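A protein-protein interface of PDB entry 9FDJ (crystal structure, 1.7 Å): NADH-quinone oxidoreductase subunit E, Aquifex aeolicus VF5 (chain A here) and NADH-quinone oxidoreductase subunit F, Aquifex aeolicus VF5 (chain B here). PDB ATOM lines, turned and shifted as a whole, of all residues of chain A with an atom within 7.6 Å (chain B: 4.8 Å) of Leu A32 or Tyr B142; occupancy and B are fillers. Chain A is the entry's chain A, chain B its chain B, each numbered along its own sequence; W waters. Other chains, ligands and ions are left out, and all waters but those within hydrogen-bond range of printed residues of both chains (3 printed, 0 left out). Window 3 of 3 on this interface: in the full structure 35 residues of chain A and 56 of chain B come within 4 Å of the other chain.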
ATOM      1  N   LYS A  15     -37.273 -15.686   8.208  1.00  0.00           N
ATOM      2  CA  LYS A  15     -35.846 -15.385   8.195  1.00  0.00           C
ATOM      3  C   LYS A  15     -35.442 -14.678   9.490  1.00  0.00           C
ATOM      4  O   LYS A  15     -34.376 -14.945  10.031  1.00  0.00           O
ATOM      5  CB  LYS A  15     -35.383 -14.542   6.998  1.00  0.00           C
ATOM      6  CG  LYS A  15     -35.609 -15.165   5.623  1.00  0.00           C
ATOM      7  CD  LYS A  15     -35.048 -14.318   4.479  1.00  0.00           C
ATOM      8  CE  LYS A  15     -35.469 -14.720   3.085  1.00  0.00           C
ATOM      9  NZ  LYS A  15     -36.864 -14.380   2.764  1.00  0.00           N
ATOM     10  N   LEU A  16     -36.294 -13.770   9.983  1.00  0.00           N
ATOM     11  CA  LEU A  16     -36.026 -13.085  11.237  1.00  0.00           C
ATOM     12  C   LEU A  16     -35.988 -14.110  12.369  1.00  0.00           C
ATOM     13  O   LEU A  16     -35.113 -14.057  13.232  1.00  0.00           O
ATOM     14  CB  LEU A  16     -37.068 -11.998  11.493  1.00  0.00           C
ATOM     15  CG  LEU A  16     -37.067 -10.831  10.503  1.00  0.00           C
ATOM     16  CD1 LEU A  16     -38.276  -9.928  10.706  1.00  0.00           C
ATOM     17  CD2 LEU A  16     -35.783 -10.038  10.609  1.00  0.00           C
ATOM     18  N   GLU A  18     -35.160 -17.248  12.141  1.00  0.00           N
ATOM     19  CA  GLU A  18     -33.917 -18.002  12.037  1.00  0.00           C
ATOM     20  C   GLU A  18     -32.770 -17.259  12.730  1.00  0.00           C
ATOM     21  O   GLU A  18     -31.970 -17.867  13.430  1.00  0.00           O
ATOM     22  CB  GLU A  18     -33.487 -18.254  10.589  1.00  0.00           C
ATOM     23  CG  GLU A  18     -34.283 -19.347   9.882  1.00  0.00           C
ATOM     24  CD  GLU A  18     -34.008 -19.411   8.386  1.00  0.00           C
ATOM     25  OE1 GLU A  18     -32.859 -19.090   8.001  1.00  0.00           O
ATOM     26  OE2 GLU A  18     -34.921 -19.787   7.613  1.00  0.00           O
ATOM     27  N   HIS A  19     -32.665 -15.948  12.518  1.00  0.00           N
ATOM     28  CA  HIS A  19     -31.611 -15.178  13.163  1.00  0.00           C
ATOM     29  C   HIS A  19     -31.806 -15.215  14.678  1.00  0.00           C
ATOM     30  O   HIS A  19     -30.857 -15.396  15.430  1.00  0.00           O
ATOM     31  CB  HIS A  19     -31.580 -13.738  12.634  1.00  0.00           C
ATOM     32  CG  HIS A  19     -31.206 -13.618  11.201  1.00  0.00           C
ATOM     33  ND1 HIS A  19     -30.091 -14.218  10.657  1.00  0.00           N
ATOM     34  CD2 HIS A  19     -31.776 -12.922  10.210  1.00  0.00           C
ATOM     35  CE1 HIS A  19     -30.032 -13.918   9.362  1.00  0.00           C
ATOM     36  NE2 HIS A  19     -31.042 -13.124   9.077  1.00  0.00           N
ATOM     37  N   ILE A  20     -33.047 -15.022  15.125  1.00  0.00           N
ATOM     38  CA  ILE A  20     -33.334 -14.909  16.547  1.00  0.00           C
ATOM     39  C   ILE A  20     -32.998 -16.225  17.246  1.00  0.00           C
ATOM     40  O   ILE A  20     -32.574 -16.200  18.395  1.00  0.00           O
ATOM     41  CB  ILE A  20     -34.792 -14.457  16.777  1.00  0.00           C
ATOM     42  CG1 ILE A  20     -34.915 -12.966  16.464  1.00  0.00           C
ATOM     43  CG2 ILE A  20     -35.270 -14.774  18.194  1.00  0.00           C
ATOM     44  CD1 ILE A  20     -36.331 -12.468  16.286  1.00  0.00           C
ATOM     45  N   TYR A  22     -30.628 -18.257  16.262  1.00  0.00           N
ATOM     46  CA  TYR A  22     -29.256 -18.633  15.936  1.00  0.00           C
ATOM     47  C   TYR A  22     -28.329 -18.486  17.144  1.00  0.00           C
ATOM     48  O   TYR A  22     -27.593 -19.416  17.453  1.00  0.00           O
ATOM     49  CB  TYR A  22     -28.759 -17.802  14.750  1.00  0.00           C
ATOM     50  CG  TYR A  22     -27.297 -17.968  14.346  1.00  0.00           C
ATOM     51  CD1 TYR A  22     -26.836 -19.109  13.687  1.00  0.00           C
ATOM     52  CD2 TYR A  22     -26.390 -16.954  14.595  1.00  0.00           C
ATOM     53  CE1 TYR A  22     -25.513 -19.235  13.301  1.00  0.00           C
ATOM     54  CE2 TYR A  22     -25.063 -17.061  14.213  1.00  0.00           C
ATOM     55  CZ  TYR A  22     -24.628 -18.194  13.550  1.00  0.00           C
ATOM     56  OH  TYR A  22     -23.326 -18.244  13.153  1.00  0.00           O
ATOM     57  N   PHE A  23     -28.309 -17.310  17.781  1.00  0.00           N
ATOM     58  CA  PHE A  23     -27.425 -17.082  18.912  1.00  0.00           C
ATOM     59  C   PHE A  23     -28.042 -17.672  20.179  1.00  0.00           C
ATOM     60  O   PHE A  23     -29.230 -18.008  20.197  1.00  0.00           O
ATOM     61  CB  PHE A  23     -27.136 -15.601  19.140  1.00  0.00           C
ATOM     62  CG  PHE A  23     -26.485 -14.881  17.977  1.00  0.00           C
ATOM     63  CD1 PHE A  23     -25.112 -14.949  17.783  1.00  0.00           C
ATOM     64  CD2 PHE A  23     -27.248 -14.119  17.102  1.00  0.00           C
ATOM     65  CE1 PHE A  23     -24.518 -14.306  16.710  1.00  0.00           C
ATOM     66  CE2 PHE A  23     -26.642 -13.473  16.034  1.00  0.00           C
ATOM     67  CZ  PHE A  23     -25.278 -13.547  15.855  1.00  0.00           C
ATOM     68  N   GLN A  28     -29.236 -10.994  20.838  1.00  0.00           N
ATOM     69  CA  GLN A  28     -27.984 -10.919  20.117  1.00  0.00           C
ATOM     70  C   GLN A  28     -28.221 -10.816  18.618  1.00  0.00           C
ATOM     71  O   GLN A  28     -27.320 -10.388  17.892  1.00  0.00           O
ATOM     72  CB  GLN A  28     -27.063 -12.101  20.398  1.00  0.00           C
ATOM     73  CG  GLN A  28     -26.798 -12.300  21.879  1.00  0.00           C
ATOM     74  CD  GLN A  28     -25.812 -13.414  22.117  1.00  0.00           C
ATOM     75  OE1 GLN A  28     -26.191 -14.525  22.495  1.00  0.00           O
ATOM     76  NE2 GLN A  28     -24.544 -13.112  21.905  1.00  0.00           N
ATOM     77  N   ALA A  29     -29.426 -11.191  18.165  1.00  0.00           N
ATOM     78  CA  ALA A  29     -29.737 -11.225  16.740  1.00  0.00           C
ATOM     79  C   ALA A  29     -30.172  -9.867  16.179  1.00  0.00           C
ATOM     80  O   ALA A  29     -30.520  -9.788  15.006  1.00  0.00           O
ATOM     81  CB  ALA A  29     -30.812 -12.254  16.497  1.00  0.00           C
ATOM     82  N   ILE A  30     -30.162  -8.799  16.991  1.00  0.00           N
ATOM     83  CA  ILE A  30     -30.754  -7.528  16.575  1.00  0.00           C
ATOM     84  C   ILE A  30     -30.155  -6.989  15.265  1.00  0.00           C
ATOM     85  O   ILE A  30     -30.899  -6.512  14.402  1.00  0.00           O
ATOM     86  CB  ILE A  30     -30.708  -6.472  17.695  1.00  0.00           C
ATOM     87  CG1 ILE A  30     -31.467  -5.201  17.272  1.00  0.00           C
ATOM     88  CG2 ILE A  30     -29.273  -6.158  18.130  1.00  0.00           C
ATOM     89  CD1 ILE A  30     -31.783  -4.264  18.418  1.00  0.00           C
ATOM     90  N   LEU A  31     -28.831  -7.012  15.097  1.00  0.00           N
ATOM     91  CA  LEU A  31     -28.233  -6.443  13.893  1.00  0.00           C
ATOM     92  C   LEU A  31     -28.499  -7.306  12.654  1.00  0.00           C
ATOM     93  O   LEU A  31     -28.711  -6.777  11.557  1.00  0.00           O
ATOM     94  CB  LEU A  31     -26.739  -6.234  14.117  1.00  0.00           C
ATOM     95  CG  LEU A  31     -26.371  -5.268  15.243  1.00  0.00           C
ATOM     96  CD1 LEU A  31     -24.884  -4.998  15.255  1.00  0.00           C
ATOM     97  CD2 LEU A  31     -27.140  -3.949  15.128  1.00  0.00           C
ATOM     98  N   LEU A  32     -28.454  -8.635  12.806  1.00  0.00           N
ATOM     99  CA  LEU A  32     -28.773  -9.522  11.700  1.00  0.00           C
ATOM    100  C   LEU A  32     -30.213  -9.278  11.247  1.00  0.00           C
ATOM    101  O   LEU A  32     -30.491  -9.260  10.046  1.00  0.00           O
ATOM    102  CB  LEU A  32     -28.535 -10.987  12.071  1.00  0.00           C
ATOM    103  CG  LEU A  32     -27.067 -11.403  12.219  1.00  0.00           C
ATOM    104  CD1 LEU A  32     -26.998 -12.837  12.694  1.00  0.00           C
ATOM    105  CD2 LEU A  32     -26.330 -11.249  10.907  1.00  0.00           C
ATOM    106  N   CYS A  33     -31.123  -9.072  12.207  1.00  0.00           N
ATOM    107  CA  CYS A  33     -32.522  -8.807  11.899  1.00  0.00           C
ATOM    108  C   CYS A  33     -32.700  -7.501  11.117  1.00  0.00           C
ATOM    109  O   CYS A  33     -33.441  -7.452  10.133  1.00  0.00           O
ATOM    110  CB  CYS A  33     -33.365  -8.794  13.162  1.00  0.00           C
ATOM    111  SG  CYS A  33     -33.653 -10.449  13.843  1.00  0.00           S
ATOM    112  N   LEU A  34     -32.008  -6.448  11.556  1.00  0.00           N
ATOM    113  CA  LEU A  34     -32.114  -5.154  10.904  1.00  0.00           C
ATOM    114  C   LEU A  34     -31.521  -5.195   9.501  1.00  0.00           C
ATOM    115  O   LEU A  34     -32.076  -4.586   8.594  1.00  0.00           O
ATOM    116  CB  LEU A  34     -31.467  -4.089  11.781  1.00  0.00           C
ATOM    117  CG  LEU A  34     -32.238  -3.781  13.067  1.00  0.00           C
ATOM    118  CD1 LEU A  34     -31.368  -2.936  13.959  1.00  0.00           C
ATOM    119  CD2 LEU A  34     -33.576  -3.087  12.809  1.00  0.00           C
ATOM    120  N   HIS A  35     -30.413  -5.921   9.308  1.00  0.00           N
ATOM    121  CA  HIS A  35     -29.866  -6.096   7.975  1.00  0.00           C
ATOM    122  C   HIS A  35     -30.894  -6.772   7.076  1.00  0.00           C
ATOM    123  O   HIS A  35     -31.086  -6.382   5.931  1.00  0.00           O
ATOM    124  CB  HIS A  35     -28.587  -6.928   8.013  1.00  0.00           C
ATOM    125  CG  HIS A  35     -27.376  -6.165   8.400  1.00  0.00           C
ATOM    126  ND1 HIS A  35     -26.903  -5.116   7.644  1.00  0.00           N
ATOM    127  CD2 HIS A  35     -26.477  -6.368   9.376  1.00  0.00           C
ATOM    128  CE1 HIS A  35     -25.763  -4.686   8.184  1.00  0.00           C
ATOM    129  NE2 HIS A  35     -25.487  -5.432   9.239  1.00  0.00           N
ATOM    130  N   GLU A  36     -31.550  -7.795   7.615  1.00  0.00           N
ATOM    131  CA  GLU A  36     -32.523  -8.564   6.867  1.00  0.00           C
ATOM    132  C   GLU A  36     -33.700  -7.676   6.452  1.00  0.00           C
ATOM    133  O   GLU A  36     -34.139  -7.716   5.300  1.00  0.00           O
ATOM    134  CB  GLU A  36     -32.917  -9.746   7.749  1.00  0.00           C
ATOM    135  CG  GLU A  36     -33.686 -10.841   7.015  1.00  0.00           C
ATOM    136  CD  GLU A  36     -32.828 -11.632   6.044  1.00  0.00           C
ATOM    137  OE1 GLU A  36     -31.775 -12.166   6.482  1.00  0.00           O
ATOM    138  OE2 GLU A  36     -33.243 -11.725   4.862  1.00  0.00           O
ATOM    139  N   ILE A  37     -34.200  -6.863   7.396  1.00  0.00           N
ATOM    140  CA  ILE A  37     -35.288  -5.933   7.119  1.00  0.00           C
ATOM    141  C   ILE A  37     -34.875  -4.918   6.045  1.00  0.00           C
ATOM    142  O   ILE A  37     -35.645  -4.661   5.125  1.00  0.00           O
ATOM    143  CB  ILE A  37     -35.769  -5.263   8.424  1.00  0.00           C
ATOM    144  CG1 ILE A  37     -36.517  -6.267   9.310  1.00  0.00           C
ATOM    145  CG2 ILE A  37     -36.629  -4.032   8.130  1.00  0.00           C
ATOM    146  CD1 ILE A  37     -36.655  -5.854  10.760  1.00  0.00           C
ATOM    147  N   GLN A  38     -33.677  -4.334   6.155  1.00  0.00           N
ATOM    148  CA  GLN A  38     -33.210  -3.373   5.169  1.00  0.00           C
ATOM    149  C   GLN A  38     -33.049  -4.029   3.795  1.00  0.00           C
ATOM    150  O   GLN A  38     -33.391  -3.433   2.771  1.00  0.00           O
ATOM    151  CB  GLN A  38     -31.903  -2.692   5.565  1.00  0.00           C
ATOM    152  CG  GLN A  38     -31.467  -1.604   4.588  1.00  0.00           C
ATOM    153  CD  GLN A  38     -30.725  -0.471   5.259  1.00  0.00           C
ATOM    154  OE1 GLN A  38     -31.277   0.251   6.096  1.00  0.00           O
ATOM    155  NE2 GLN A  38     -29.460  -0.308   4.910  1.00  0.00           N
ATOM    156  N   LEU A  52     -40.406  -6.022  15.524  1.00  0.00           N
ATOM    157  CA  LEU A  52     -39.071  -6.576  15.715  1.00  0.00           C
ATOM    158  C   LEU A  52     -38.763  -6.640  17.208  1.00  0.00           C
ATOM    159  O   LEU A  52     -38.308  -7.666  17.709  1.00  0.00           O
ATOM    160  CB  LEU A  52     -37.996  -5.785  14.970  1.00  0.00           C
ATOM    161  CG  LEU A  52     -36.552  -6.230  15.223  1.00  0.00           C
ATOM    162  CD1 LEU A  52     -36.387  -7.701  14.874  1.00  0.00           C
ATOM    163  CD2 LEU A  52     -35.566  -5.370  14.462  1.00  0.00           C
ATOM    164  N   PHE A  73     -27.706   1.446   8.562  1.00  0.00           N
ATOM    165  CA  PHE A  73     -29.158   1.412   8.505  1.00  0.00           C
ATOM    166  C   PHE A  73     -29.693   2.782   8.117  1.00  0.00           C
ATOM    167  O   PHE A  73     -29.183   3.793   8.594  1.00  0.00           O
ATOM    168  CB  PHE A  73     -29.754   0.968   9.837  1.00  0.00           C
ATOM    169  CG  PHE A  73     -29.279  -0.407  10.277  1.00  0.00           C
ATOM    170  CD1 PHE A  73     -29.245  -1.468   9.376  1.00  0.00           C
ATOM    171  CD2 PHE A  73     -28.818  -0.616  11.573  1.00  0.00           C
ATOM    172  CE1 PHE A  73     -28.774  -2.710   9.768  1.00  0.00           C
ATOM    173  CE2 PHE A  73     -28.368  -1.869  11.963  1.00  0.00           C
ATOM    174  CZ  PHE A  73     -28.345  -2.905  11.059  1.00  0.00           C
ATOM    175  N   ASP A 141     -24.185  -5.623  -1.820  1.00  0.00           N
ATOM    176  CA  ASP A 141     -23.101  -6.398  -1.230  1.00  0.00           C
ATOM    177  C   ASP A 141     -21.886  -6.536  -2.151  1.00  0.00           C
ATOM    178  O   ASP A 141     -20.827  -6.986  -1.711  1.00  0.00           O
ATOM    179  CB  ASP A 141     -23.564  -7.787  -0.837  1.00  0.00           C
ATOM    180  CG  ASP A 141     -24.454  -7.858   0.397  1.00  0.00           C
ATOM    181  OD1 ASP A 141     -24.654  -6.811   1.031  1.00  0.00           O
ATOM    182  OD2 ASP A 141     -24.944  -8.973   0.688  1.00  0.00           O
ATOM    183  N   ILE B 134     -17.752  -9.749  12.527  1.00  0.00           N
ATOM    184  CA  ILE B 134     -17.237  -9.234  11.264  1.00  0.00           C
ATOM    185  C   ILE B 134     -18.005  -7.965  10.903  1.00  0.00           C
ATOM    186  O   ILE B 134     -19.236  -7.908  11.004  1.00  0.00           O
ATOM    187  CB  ILE B 134     -17.266 -10.304  10.157  1.00  0.00           C
ATOM    188  CG1 ILE B 134     -16.562  -9.796   8.890  1.00  0.00           C
ATOM    189  CG2 ILE B 134     -18.679 -10.803   9.845  1.00  0.00           C
ATOM    190  CD1 ILE B 134     -16.316 -10.869   7.844  1.00  0.00           C
ATOM    191  N   TYR B 138     -18.320  -6.174   5.162  1.00  0.00           N
ATOM    192  CA  TYR B 138     -17.683  -7.375   4.646  1.00  0.00           C
ATOM    193  C   TYR B 138     -18.737  -8.479   4.455  1.00  0.00           C
ATOM    194  O   TYR B 138     -18.680  -9.562   5.087  1.00  0.00           O
ATOM    195  CB  TYR B 138     -16.559  -7.867   5.561  1.00  0.00           C
ATOM    196  CG  TYR B 138     -15.235  -7.112   5.611  1.00  0.00           C
ATOM    197  CD1 TYR B 138     -14.909  -6.106   4.694  1.00  0.00           C
ATOM    198  CD2 TYR B 138     -14.278  -7.449   6.551  1.00  0.00           C
ATOM    199  CE1 TYR B 138     -13.685  -5.460   4.741  1.00  0.00           C
ATOM    200  CE2 TYR B 138     -13.049  -6.813   6.602  1.00  0.00           C
ATOM    201  CZ  TYR B 138     -12.745  -5.820   5.686  1.00  0.00           C
ATOM    202  OH  TYR B 138     -11.517  -5.220   5.745  1.00  0.00           O
ATOM    203  N   PRO B 139     -19.739  -8.282   3.568  1.00  0.00           N
ATOM    204  CA  PRO B 139     -20.788  -9.285   3.404  1.00  0.00           C
ATOM    205  C   PRO B 139     -20.286 -10.601   2.832  1.00  0.00           C
ATOM    206  O   PRO B 139     -20.734 -11.665   3.245  1.00  0.00           O
ATOM    207  CB  PRO B 139     -21.813  -8.630   2.507  1.00  0.00           C
ATOM    208  CG  PRO B 139     -21.001  -7.628   1.720  1.00  0.00           C
ATOM    209  CD  PRO B 139     -19.959  -7.116   2.702  1.00  0.00           C
ATOM    210  N   ALA B 140     -19.358 -10.537   1.879  1.00  0.00           N
ATOM    211  CA  ALA B 140     -18.818 -11.762   1.305  1.00  0.00           C
ATOM    212  C   ALA B 140     -18.085 -12.566   2.372  1.00  0.00           C
ATOM    213  O   ALA B 140     -18.261 -13.776   2.444  1.00  0.00           O
ATOM    214  CB  ALA B 140     -17.924 -11.451   0.125  1.00  0.00           C
ATOM    215  N   GLY B 141     -17.256 -11.906   3.194  1.00  0.00           N
ATOM    216  CA  GLY B 141     -16.541 -12.586   4.262  1.00  0.00           C
ATOM    217  C   GLY B 141     -17.494 -13.289   5.219  1.00  0.00           C
ATOM    218  O   GLY B 141     -17.247 -14.420   5.658  1.00  0.00           O
ATOM    219  N   TYR B 142     -18.614 -12.617   5.510  1.00  0.00           N
ATOM    220  CA  TYR B 142     -19.643 -13.200   6.354  1.00  0.00           C
ATOM    221  C   TYR B 142     -20.154 -14.517   5.760  1.00  0.00           C
ATOM    222  O   TYR B 142     -20.126 -15.542   6.439  1.00  0.00           O
ATOM    223  CB  TYR B 142     -20.777 -12.196   6.570  1.00  0.00           C
ATOM    224  CG  TYR B 142     -21.974 -12.829   7.250  1.00  0.00           C
ATOM    225  CD1 TYR B 142     -21.992 -13.021   8.633  1.00  0.00           C
ATOM    226  CD2 TYR B 142     -23.097 -13.195   6.528  1.00  0.00           C
ATOM    227  CE1 TYR B 142     -23.081 -13.610   9.261  1.00  0.00           C
ATOM    228  CE2 TYR B 142     -24.196 -13.766   7.144  1.00  0.00           C
ATOM    229  CZ  TYR B 142     -24.191 -13.972   8.511  1.00  0.00           C
ATOM    230  OH  TYR B 142     -25.294 -14.551   9.076  1.00  0.00           O
ATOM    231  N   TYR B 143     -20.598 -14.502   4.493  1.00  0.00           N
ATOM    232  CA  TYR B 143     -21.159 -15.698   3.861  1.00  0.00           C
ATOM    233  C   TYR B 143     -20.094 -16.789   3.722  1.00  0.00           C
ATOM    234  O   TYR B 143     -20.386 -17.974   3.939  1.00  0.00           O
ATOM    235  CB  TYR B 143     -21.837 -15.361   2.530  1.00  0.00           C
ATOM    236  CG  TYR B 143     -23.053 -14.453   2.686  1.00  0.00           C
ATOM    237  CD1 TYR B 143     -24.162 -14.885   3.404  1.00  0.00           C
ATOM    238  CD2 TYR B 143     -23.092 -13.177   2.135  1.00  0.00           C
ATOM    239  CE1 TYR B 143     -25.267 -14.076   3.585  1.00  0.00           C
ATOM    240  CE2 TYR B 143     -24.203 -12.357   2.299  1.00  0.00           C
ATOM    241  CZ  TYR B 143     -25.278 -12.800   3.054  1.00  0.00           C
ATOM    242  OH  TYR B 143     -26.390 -12.039   3.257  1.00  0.00           O
ATOM    243  N   ILE B 144     -18.859 -16.384   3.411  1.00  0.00           N
ATOM    244  CA  ILE B 144     -17.745 -17.321   3.286  1.00  0.00           C
ATOM    245  C   ILE B 144     -17.492 -18.040   4.605  1.00  0.00           C
ATOM    246  O   ILE B 144     -17.359 -19.271   4.621  1.00  0.00           O
ATOM    247  CB  ILE B 144     -16.496 -16.612   2.748  1.00  0.00           C
ATOM    248  CG1 ILE B 144     -16.737 -16.238   1.271  1.00  0.00           C
ATOM    249  CG2 ILE B 144     -15.248 -17.486   2.927  1.00  0.00           C
ATOM    250  CD1 ILE B 144     -15.796 -15.193   0.711  1.00  0.00           C
ATOM    251  N   LEU B 145     -17.479 -17.279   5.703  1.00  0.00           N
ATOM    252  CA  LEU B 145     -17.273 -17.857   7.023  1.00  0.00           C
ATOM    253  C   LEU B 145     -18.424 -18.778   7.416  1.00  0.00           C
ATOM    254  O   LEU B 145     -18.175 -19.843   7.974  1.00  0.00           O
ATOM    255  CB  LEU B 145     -17.074 -16.766   8.081  1.00  0.00           C
ATOM    256  CG  LEU B 145     -15.735 -16.044   8.030  1.00  0.00           C
ATOM    257  CD1 LEU B 145     -15.796 -14.810   8.892  1.00  0.00           C
ATOM    258  CD2 LEU B 145     -14.606 -16.972   8.434  1.00  0.00           C
ATOM    259  N   ARG B 146     -19.679 -18.373   7.154  1.00  0.00           N
ATOM    260  CA  ARG B 146     -20.817 -19.190   7.543  1.00  0.00           C
ATOM    261  C   ARG B 146     -20.681 -20.555   6.870  1.00  0.00           C
ATOM    262  O   ARG B 146     -20.898 -21.606   7.489  1.00  0.00           O
ATOM    263  CB  ARG B 146     -22.195 -18.570   7.240  1.00  0.00           C
ATOM    264  CG  ARG B 146     -22.663 -17.428   8.130  1.00  0.00           C
ATOM    265  CD  ARG B 146     -22.930 -17.859   9.564  1.00  0.00           C
ATOM    266  NE  ARG B 146     -23.931 -18.930   9.654  1.00  0.00           N
ATOM    267  CZ  ARG B 146     -25.258 -18.788   9.695  1.00  0.00           C
ATOM    268  NH1 ARG B 146     -25.806 -17.607   9.889  1.00  0.00           N
ATOM    269  NH2 ARG B 146     -26.045 -19.854   9.625  1.00  0.00           N
ATOM    270  N   VAL B 173     -21.371 -16.438  14.084  1.00  0.00           N
ATOM    271  CA  VAL B 173     -20.901 -15.293  13.323  1.00  0.00           C
ATOM    272  C   VAL B 173     -21.904 -14.152  13.475  1.00  0.00           C
ATOM    273  O   VAL B 173     -23.073 -14.284  13.080  1.00  0.00           O
ATOM    274  CB  VAL B 173     -20.657 -15.618  11.839  1.00  0.00           C
ATOM    275  CG1 VAL B 173     -19.951 -14.469  11.136  1.00  0.00           C
ATOM    276  CG2 VAL B 173     -19.885 -16.923  11.635  1.00  0.00           C
ATOM    277  N   ARG B 175     -22.529  -9.846  12.758  1.00  0.00           N
ATOM    278  CA  ARG B 175     -22.183  -8.797  11.814  1.00  0.00           C
ATOM    279  C   ARG B 175     -22.342  -7.454  12.505  1.00  0.00           C
ATOM    280  O   ARG B 175     -23.307  -7.231  13.243  1.00  0.00           O
ATOM    281  CB  ARG B 175     -23.110  -8.796  10.597  1.00  0.00           C
ATOM    282  CG  ARG B 175     -23.008 -10.066   9.771  1.00  0.00           C
ATOM    283  CD  ARG B 175     -23.891  -9.985   8.537  1.00  0.00           C
ATOM    284  NE  ARG B 175     -23.443  -8.998   7.553  1.00  0.00           N
ATOM    285  CZ  ARG B 175     -24.157  -8.538   6.524  1.00  0.00           C
ATOM    286  NH1 ARG B 175     -25.393  -8.945   6.302  1.00  0.00           N
ATOM    287  NH2 ARG B 175     -23.636  -7.634   5.707  1.00  0.00           N
HETATM  288  O   HOH W   1     -28.019 -15.804  11.763  1.00  0.00           O
HETATM  289  O   HOH W   2     -26.256  -9.497   2.892  1.00  0.00           O
HETATM  290  O   HOH W   3     -25.094  -6.340   3.574  1.00  0.00           O
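The side-chain hydroxyl (OH) of Tyr A22 sits at hydrogen-bond distance from the backbone NH (N) of Val B173.
The side-chain hydroxyl (OH) of Tyr B142 sits at hydrogen-bond distance from the guanidinium group (NH1) of Arg B146 (3.2 Å).
Tyr A22 touches Arg B146 (OH to NE, 3.6 Å).
Phe A23 touches Val B173.
CD1 of Leu A31 touches O of Arg B175 (3.4 Å).
Tyr B142 touches Leu A32.
Arg B175 touches Leu A32.
Pro B139 touches Asp A141 (CB to CG, 3.5 Å).
Asp A141 touches Tyr B143 (OD2 to CE2, 3.8 Å).
Of the printed residues of chain B, Tyr A22 touches Arg B146 and Val B173.
Printed residues of chain B within 4 Å of Leu A31: Arg B175.
Of chain B, only Tyr B142 (3.9 Å) and Arg B175 (3.6 Å) come within 4 Å of Leu A32.
Of chain A, only Leu A32 comes within 4 Å of Tyr B142.
The nearest residue of chain B that does not touch Leu A32 is Val B173 (4.2 Å).
The nearest residue of chain A that does not touch Tyr B142 is His A19 (4.8 Å).
Of the 21 printed residues of chain A, 5 touch a printed residue of chain B.
Hydrophobic or aromatic side chains of chain A that line the printed part of chain B: Tyr A22, Phe A23, Leu A31 and Leu A32.
Of the 12 printed residues of chain B, 6 touch a printed residue of chain A.
Printed residues of chain B that touch a printed residue of chain A: Pro B139, Tyr B142, Tyr B143, Arg B146, Val B173 and Arg B175.
Among the printed residues, no Asp or Glu carboxylate lies within 4 Å of a Lys or Arg side-chain nitrogen of the other chain.
Water W2 bridges the side-chain hydroxyl of Tyr B143 (2.6 Å) and the side-chain carboxylate of Asp A141 (2.6 Å).
Water W3 lies within hydrogen-bond range of the side-chain carboxylate of Asp A141 and the guanidinium group of Arg B175.
Water W1 lies within hydrogen-bond range of ND1 of His A19 and NH1 of Arg B146.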
